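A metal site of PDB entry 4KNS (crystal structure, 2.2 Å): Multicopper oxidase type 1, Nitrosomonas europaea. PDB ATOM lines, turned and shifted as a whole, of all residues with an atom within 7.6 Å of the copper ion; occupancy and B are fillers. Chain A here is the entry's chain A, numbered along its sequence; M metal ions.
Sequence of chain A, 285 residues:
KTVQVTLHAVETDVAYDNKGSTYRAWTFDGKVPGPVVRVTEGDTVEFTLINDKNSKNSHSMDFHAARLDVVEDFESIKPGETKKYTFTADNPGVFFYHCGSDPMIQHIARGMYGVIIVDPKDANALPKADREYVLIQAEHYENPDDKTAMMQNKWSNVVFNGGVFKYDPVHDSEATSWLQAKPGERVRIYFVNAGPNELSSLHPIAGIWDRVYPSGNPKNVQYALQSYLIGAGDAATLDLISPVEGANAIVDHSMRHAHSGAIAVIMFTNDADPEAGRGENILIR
The backbone NH (N) of Ser 101 lies close to the side-chain sulfur (SG) of Cys 99. The backbone NH (N) of His 59 sits close to the side-chain amide nitrogen (ND2) of Asn 51 (3.4 Å). NE2 of His 59 lies close to O of Asn 57, 3.4 Å away. A ring nitrogen (NE2) of His 107 lies within hydrogen-bond range of the backbone carbonyl oxygen of Asp 102. NE2 of His 59 lies within hydrogen-bond range of OE2 of Glu 11. The side-chain sulfur (SG) of Cys 99 sits close to the backbone NH (N) of Ser 60 (3.3 Å). N of Met 112 sits at hydrogen-bond distance from O of Trp 26 (3.1 Å).
Four residues have an atom within 4 Å of the copper ion: His 59, Cys 99, His 107 and Met 112. The nearest printed residue that does not touch the copper ion is Ser 58 (4.1 Å).
The copper ion is bound by a ring nitrogen (ND1) of His 59 (2.1 Å). ND1 of His 107 is bound to the copper ion. SG of Cys 99 is bound to the copper ion (2.3 Å). The copper ion is bound by the side-chain sulfur (SD) of Met 112 (2.4 Å).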
ATOM      1  N   ALA A   9      -3.144  10.665 -12.664  1.00  0.00           N
ATOM      2  CA  ALA A   9      -3.187   9.290 -12.169  1.00  0.00           C
ATOM      3  C   ALA A   9      -4.588   8.730 -12.408  1.00  0.00           C
ATOM      4  O   ALA A   9      -5.556   9.148 -11.758  1.00  0.00           O
ATOM      5  CB  ALA A   9      -2.822   9.225 -10.705  1.00  0.00           C
ATOM      6  N   GLU A  11      -7.070   5.306 -12.873  1.00  0.00           N
ATOM      7  CA  GLU A  11      -7.313   3.881 -12.659  1.00  0.00           C
ATOM      8  C   GLU A  11      -8.437   3.406 -13.586  1.00  0.00           C
ATOM      9  O   GLU A  11      -9.610   3.707 -13.369  1.00  0.00           O
ATOM     10  CB  GLU A  11      -7.674   3.597 -11.195  1.00  0.00           C
ATOM     11  CG  GLU A  11      -6.613   4.052 -10.201  1.00  0.00           C
ATOM     12  CD  GLU A  11      -7.015   3.864  -8.759  1.00  0.00           C
ATOM     13  OE1 GLU A  11      -8.128   3.365  -8.482  1.00  0.00           O
ATOM     14  OE2 GLU A  11      -6.209   4.214  -7.869  1.00  0.00           O
ATOM     15  N   TRP A  26      -3.543   0.653 -13.142  1.00  0.00           N
ATOM     16  CA  TRP A  26      -3.266   1.988 -12.649  1.00  0.00           C
ATOM     17  C   TRP A  26      -2.334   2.635 -13.628  1.00  0.00           C
ATOM     18  O   TRP A  26      -1.310   2.054 -13.999  1.00  0.00           O
ATOM     19  CB  TRP A  26      -2.648   1.953 -11.251  1.00  0.00           C
ATOM     20  CG  TRP A  26      -3.484   1.253 -10.206  1.00  0.00           C
ATOM     21  CD1 TRP A  26      -4.849   0.968 -10.249  1.00  0.00           C
ATOM     22  CD2 TRP A  26      -3.040   0.750  -8.896  1.00  0.00           C
ATOM     23  NE1 TRP A  26      -5.258   0.331  -9.110  1.00  0.00           N
ATOM     24  CE2 TRP A  26      -4.220   0.168  -8.256  1.00  0.00           C
ATOM     25  CE3 TRP A  26      -1.825   0.717  -8.226  1.00  0.00           C
ATOM     26  CZ2 TRP A  26      -4.157  -0.407  -6.994  1.00  0.00           C
ATOM     27  CZ3 TRP A  26      -1.778   0.134  -6.955  1.00  0.00           C
ATOM     28  CH2 TRP A  26      -2.919  -0.422  -6.356  1.00  0.00           C
ATOM     29  N   THR A  27      -2.690   3.844 -14.075  1.00  0.00           N
ATOM     30  CA  THR A  27      -2.027   4.452 -15.228  1.00  0.00           C
ATOM     31  C   THR A  27      -1.730   5.941 -15.049  1.00  0.00           C
ATOM     32  O   THR A  27      -2.296   6.608 -14.182  1.00  0.00           O
ATOM     33  CB  THR A  27      -2.869   4.335 -16.514  1.00  0.00           C
ATOM     34  OG1 THR A  27      -3.920   5.314 -16.485  1.00  0.00           O
ATOM     35  CG2 THR A  27      -3.477   2.951 -16.684  1.00  0.00           C
ATOM     36  N   PHE A  28      -0.846   6.442 -15.900  1.00  0.00           N
ATOM     37  CA  PHE A  28      -0.739   7.862 -16.168  1.00  0.00           C
ATOM     38  C   PHE A  28      -1.482   8.167 -17.467  1.00  0.00           C
ATOM     39  O   PHE A  28      -1.211   7.543 -18.497  1.00  0.00           O
ATOM     40  CB  PHE A  28       0.721   8.309 -16.249  1.00  0.00           C
ATOM     41  CG  PHE A  28       1.473   8.161 -14.964  1.00  0.00           C
ATOM     42  CD1 PHE A  28       1.189   8.977 -13.869  1.00  0.00           C
ATOM     43  CD2 PHE A  28       2.479   7.214 -14.830  1.00  0.00           C
ATOM     44  CE1 PHE A  28       1.887   8.850 -12.674  1.00  0.00           C
ATOM     45  CE2 PHE A  28       3.189   7.078 -13.645  1.00  0.00           C
ATOM     46  CZ  PHE A  28       2.889   7.897 -12.573  1.00  0.00           C
ATOM     47  N   LEU A  49       1.142  16.678 -11.055  1.00  0.00           N
ATOM     48  CA  LEU A  49       0.421  15.411 -10.969  1.00  0.00           C
ATOM     49  C   LEU A  49      -0.954  15.611 -10.331  1.00  0.00           C
ATOM     50  O   LEU A  49      -1.074  16.123  -9.219  1.00  0.00           O
ATOM     51  CB  LEU A  49       1.206  14.360 -10.196  1.00  0.00           C
ATOM     52  CG  LEU A  49       0.518  13.009  -9.944  1.00  0.00           C
ATOM     53  CD1 LEU A  49       0.401  12.180 -11.214  1.00  0.00           C
ATOM     54  CD2 LEU A  49       1.235  12.233  -8.852  1.00  0.00           C
ATOM     55  N   ASN A  51      -4.114  13.457  -9.121  1.00  0.00           N
ATOM     56  CA  ASN A  51      -4.734  12.175  -8.823  1.00  0.00           C
ATOM     57  C   ASN A  51      -6.253  12.307  -8.955  1.00  0.00           C
ATOM     58  O   ASN A  51      -6.890  13.021  -8.181  1.00  0.00           O
ATOM     59  CB  ASN A  51      -4.344  11.691  -7.414  1.00  0.00           C
ATOM     60  CG  ASN A  51      -4.620  10.209  -7.201  1.00  0.00           C
ATOM     61  OD1 ASN A  51      -5.194   9.525  -8.056  1.00  0.00           O
ATOM     62  ND2 ASN A  51      -4.213   9.698  -6.040  1.00  0.00           N
ATOM     63  N   ASN A  57      -6.787   4.782  -4.775  1.00  0.00           N
ATOM     64  CA  ASN A  57      -5.445   4.662  -4.210  1.00  0.00           C
ATOM     65  C   ASN A  57      -4.671   5.977  -4.292  1.00  0.00           C
ATOM     66  O   ASN A  57      -4.920   6.793  -5.183  1.00  0.00           O
ATOM     67  CB  ASN A  57      -4.658   3.571  -4.949  1.00  0.00           C
ATOM     68  CG  ASN A  57      -5.372   2.230  -4.937  1.00  0.00           C
ATOM     69  OD1 ASN A  57      -5.205   1.425  -4.022  1.00  0.00           O
ATOM     70  ND2 ASN A  57      -6.162   1.985  -5.981  1.00  0.00           N
ATOM     71  N   SER A  58      -3.750   6.163  -3.361  1.00  0.00           N
ATOM     72  CA  SER A  58      -2.816   7.287  -3.419  1.00  0.00           C
ATOM     73  C   SER A  58      -1.722   7.010  -4.450  1.00  0.00           C
ATOM     74  O   SER A  58      -1.261   5.877  -4.582  1.00  0.00           O
ATOM     75  CB  SER A  58      -2.197   7.552  -2.049  1.00  0.00           C
ATOM     76  OG  SER A  58      -3.171   8.089  -1.158  1.00  0.00           O
ATOM     77  N   HIS A  59      -1.332   8.056  -5.177  1.00  0.00           N
ATOM     78  CA  HIS A  59      -0.330   7.938  -6.238  1.00  0.00           C
ATOM     79  C   HIS A  59       0.706   9.010  -6.156  1.00  0.00           C
ATOM     80  O   HIS A  59       0.493  10.048  -5.524  1.00  0.00           O
ATOM     81  CB  HIS A  59      -0.995   7.948  -7.606  1.00  0.00           C
ATOM     82  CG  HIS A  59      -1.987   6.829  -7.826  1.00  0.00           C
ATOM     83  ND1 HIS A  59      -1.626   5.546  -7.916  1.00  0.00           N
ATOM     84  CD2 HIS A  59      -3.376   6.857  -7.965  1.00  0.00           C
ATOM     85  CE1 HIS A  59      -2.711   4.776  -8.103  1.00  0.00           C
ATOM     86  NE2 HIS A  59      -3.781   5.580  -8.132  1.00  0.00           N
ATOM     87  N   SER A  60       1.849   8.770  -6.786  1.00  0.00           N
ATOM     88  CA  SER A  60       2.967   9.711  -6.792  1.00  0.00           C
ATOM     89  C   SER A  60       3.710   9.644  -8.118  1.00  0.00           C
ATOM     90  O   SER A  60       3.302   8.908  -9.023  1.00  0.00           O
ATOM     91  CB  SER A  60       3.917   9.414  -5.634  1.00  0.00           C
ATOM     92  OG  SER A  60       4.341   8.067  -5.680  1.00  0.00           O
ATOM     93  N   MET A  61       4.797  10.406  -8.227  1.00  0.00           N
ATOM     94  CA  MET A  61       5.618  10.387  -9.429  1.00  0.00           C
ATOM     95  C   MET A  61       7.115  10.464  -9.129  1.00  0.00           C
ATOM     96  O   MET A  61       7.566  11.352  -8.417  1.00  0.00           O
ATOM     97  CB  MET A  61       5.223  11.513 -10.384  1.00  0.00           C
ATOM     98  CG  MET A  61       6.151  11.661 -11.580  1.00  0.00           C
ATOM     99  SD  MET A  61       6.137  10.244 -12.702  1.00  0.00           S
ATOM    100  CE  MET A  61       4.803  10.726 -13.791  1.00  0.00           C
ATOM    101  N   SER A  76       3.283  10.434  -1.900  1.00  0.00           N
ATOM    102  CA  SER A  76       1.980  10.001  -2.390  1.00  0.00           C
ATOM    103  C   SER A  76       0.901  11.056  -2.109  1.00  0.00           C
ATOM    104  O   SER A  76       0.910  11.694  -1.054  1.00  0.00           O
ATOM    105  CB  SER A  76       1.556   8.677  -1.732  1.00  0.00           C
ATOM    106  OG  SER A  76       2.499   7.656  -1.993  1.00  0.00           O
ATOM    107  N   HIS A  98       8.142   6.467 -13.035  1.00  0.00           N
ATOM    108  CA  HIS A  98       7.122   5.592 -12.460  1.00  0.00           C
ATOM    109  C   HIS A  98       6.523   6.146 -11.204  1.00  0.00           C
ATOM    110  O   HIS A  98       7.060   7.078 -10.607  1.00  0.00           O
ATOM    111  CB  HIS A  98       7.710   4.203 -12.175  1.00  0.00           C
ATOM    112  CG  HIS A  98       8.821   4.218 -11.153  1.00  0.00           C
ATOM    113  ND1 HIS A  98       8.595   3.985  -9.845  1.00  0.00           N
ATOM    114  CD2 HIS A  98      10.183   4.452 -11.285  1.00  0.00           C
ATOM    115  CE1 HIS A  98       9.766   4.055  -9.176  1.00  0.00           C
ATOM    116  NE2 HIS A  98      10.735   4.344 -10.058  1.00  0.00           N
ATOM    117  N   CYS A  99       5.403   5.558 -10.787  1.00  0.00           N
ATOM    118  CA  CYS A  99       4.802   5.871  -9.496  1.00  0.00           C
ATOM    119  C   CYS A  99       5.641   5.284  -8.354  1.00  0.00           C
ATOM    120  O   CYS A  99       6.165   4.174  -8.468  1.00  0.00           O
ATOM    121  CB  CYS A  99       3.380   5.335  -9.434  1.00  0.00           C
ATOM    122  SG  CYS A  99       2.490   5.742  -7.918  1.00  0.00           S
ATOM    123  N   GLY A 100       5.755   6.032  -7.264  1.00  0.00           N
ATOM    124  CA  GLY A 100       6.557   5.618  -6.113  1.00  0.00           C
ATOM    125  C   GLY A 100       5.772   5.320  -4.842  1.00  0.00           C
ATOM    126  O   GLY A 100       6.351   5.291  -3.752  1.00  0.00           O
ATOM    127  N   SER A 101       4.477   5.100  -4.986  1.00  0.00           N
ATOM    128  CA  SER A 101       3.584   4.867  -3.850  1.00  0.00           C
ATOM    129  C   SER A 101       3.626   3.429  -3.316  1.00  0.00           C
ATOM    130  O   SER A 101       4.094   2.528  -4.005  1.00  0.00           O
ATOM    131  CB  SER A 101       2.142   5.260  -4.212  1.00  0.00           C
ATOM    132  OG  SER A 101       2.064   6.649  -4.450  1.00  0.00           O
ATOM    133  N   ASP A 102       3.120   3.245  -2.103  1.00  0.00           N
ATOM    134  CA  ASP A 102       3.203   1.968  -1.382  1.00  0.00           C
ATOM    135  C   ASP A 102       2.113   0.998  -1.837  1.00  0.00           C
ATOM    136  O   ASP A 102       0.929   1.342  -1.848  1.00  0.00           O
ATOM    137  CB  ASP A 102       3.107   2.221   0.124  1.00  0.00           C
ATOM    138  CG  ASP A 102       3.574   1.030   0.971  1.00  0.00           C
ATOM    139  OD1 ASP A 102       4.604   0.401   0.633  1.00  0.00           O
ATOM    140  OD2 ASP A 102       2.912   0.736   1.985  1.00  0.00           O
ATOM    141  N   PRO A 103       2.499  -0.234  -2.257  1.00  0.00           N
ATOM    142  CA  PRO A 103       3.884  -0.660  -2.496  1.00  0.00           C
ATOM    143  C   PRO A 103       4.288  -0.450  -3.955  1.00  0.00           C
ATOM    144  O   PRO A 103       3.513  -0.753  -4.860  1.00  0.00           O
ATOM    145  CB  PRO A 103       3.850  -2.147  -2.148  1.00  0.00           C
ATOM    146  CG  PRO A 103       2.436  -2.576  -2.416  1.00  0.00           C
ATOM    147  CD  PRO A 103       1.559  -1.355  -2.375  1.00  0.00           C
ATOM    148  N   MET A 104       5.498   0.067  -4.166  1.00  0.00           N
ATOM    149  CA  MET A 104       6.006   0.383  -5.512  1.00  0.00           C
ATOM    150  C   MET A 104       5.895  -0.786  -6.488  1.00  0.00           C
ATOM    151  O   MET A 104       5.568  -0.592  -7.654  1.00  0.00           O
ATOM    152  CB  MET A 104       7.456   0.865  -5.453  1.00  0.00           C
ATOM    153  CG  MET A 104       7.602   2.351  -5.163  1.00  0.00           C
ATOM    154  SD  MET A 104       9.261   2.968  -5.525  1.00  0.00           S
ATOM    155  CE  MET A 104      10.114   2.576  -4.002  1.00  0.00           C
ATOM    156  N   GLN A 106       3.631  -3.047  -6.748  1.00  0.00           N
ATOM    157  CA  GLN A 106       2.277  -3.142  -7.294  1.00  0.00           C
ATOM    158  C   GLN A 106       1.958  -1.977  -8.219  1.00  0.00           C
ATOM    159  O   GLN A 106       1.311  -2.162  -9.252  1.00  0.00           O
ATOM    160  CB  GLN A 106       1.239  -3.233  -6.163  1.00  0.00           C
ATOM    161  CG  GLN A 106      -0.154  -3.614  -6.645  1.00  0.00           C
ATOM    162  CD  GLN A 106      -1.210  -3.561  -5.563  1.00  0.00           C
ATOM    163  OE1 GLN A 106      -1.049  -2.872  -4.554  1.00  0.00           O
ATOM    164  NE2 GLN A 106      -2.308  -4.282  -5.769  1.00  0.00           N
ATOM    165  N   HIS A 107       2.398  -0.783  -7.862  1.00  0.00           N
ATOM    166  CA  HIS A 107       2.125   0.417  -8.660  1.00  0.00           C
ATOM    167  C   HIS A 107       2.774   0.363 -10.023  1.00  0.00           C
ATOM    168  O   HIS A 107       2.156   0.733 -11.021  1.00  0.00           O
ATOM    169  CB  HIS A 107       2.512   1.690  -7.922  1.00  0.00           C
ATOM    170  CG  HIS A 107       1.545   2.061  -6.812  1.00  0.00           C
ATOM    171  ND1 HIS A 107       0.509   2.889  -7.017  1.00  0.00           N
ATOM    172  CD2 HIS A 107       1.485   1.672  -5.480  1.00  0.00           C
ATOM    173  CE1 HIS A 107      -0.184   3.023  -5.864  1.00  0.00           C
ATOM    174  NE2 HIS A 107       0.418   2.284  -4.922  1.00  0.00           N
ATOM    175  N   ILE A 108       4.006  -0.134 -10.088  1.00  0.00           N
ATOM    176  CA  ILE A 108       4.693  -0.353 -11.367  1.00  0.00           C
ATOM    177  C   ILE A 108       4.021  -1.476 -12.160  1.00  0.00           C
ATOM    178  O   ILE A 108       3.718  -1.298 -13.344  1.00  0.00           O
ATOM    179  CB  ILE A 108       6.200  -0.646 -11.167  1.00  0.00           C
ATOM    180  CG1 ILE A 108       6.899   0.556 -10.512  1.00  0.00           C
ATOM    181  CG2 ILE A 108       6.871  -0.992 -12.501  1.00  0.00           C
ATOM    182  CD1 ILE A 108       8.226   0.218  -9.850  1.00  0.00           C
ATOM    183  N   MET A 112       1.825   1.873 -13.904  1.00  0.00           N
ATOM    184  CA  MET A 112       2.223   3.260 -13.651  1.00  0.00           C
ATOM    185  C   MET A 112       3.698   3.485 -13.965  1.00  0.00           C
ATOM    186  O   MET A 112       4.501   3.712 -13.061  1.00  0.00           O
ATOM    187  CB  MET A 112       1.888   3.689 -12.229  1.00  0.00           C
ATOM    188  CG  MET A 112       0.420   3.582 -11.863  1.00  0.00           C
ATOM    189  SD  MET A 112      -0.122   4.622 -10.505  1.00  0.00           S
ATOM    190  CE  MET A 112      -0.235   6.214 -11.308  1.00  0.00           C
HETATM  191 CU    CU M   1       0.368   4.819  -8.193  1.00  0.00          CU
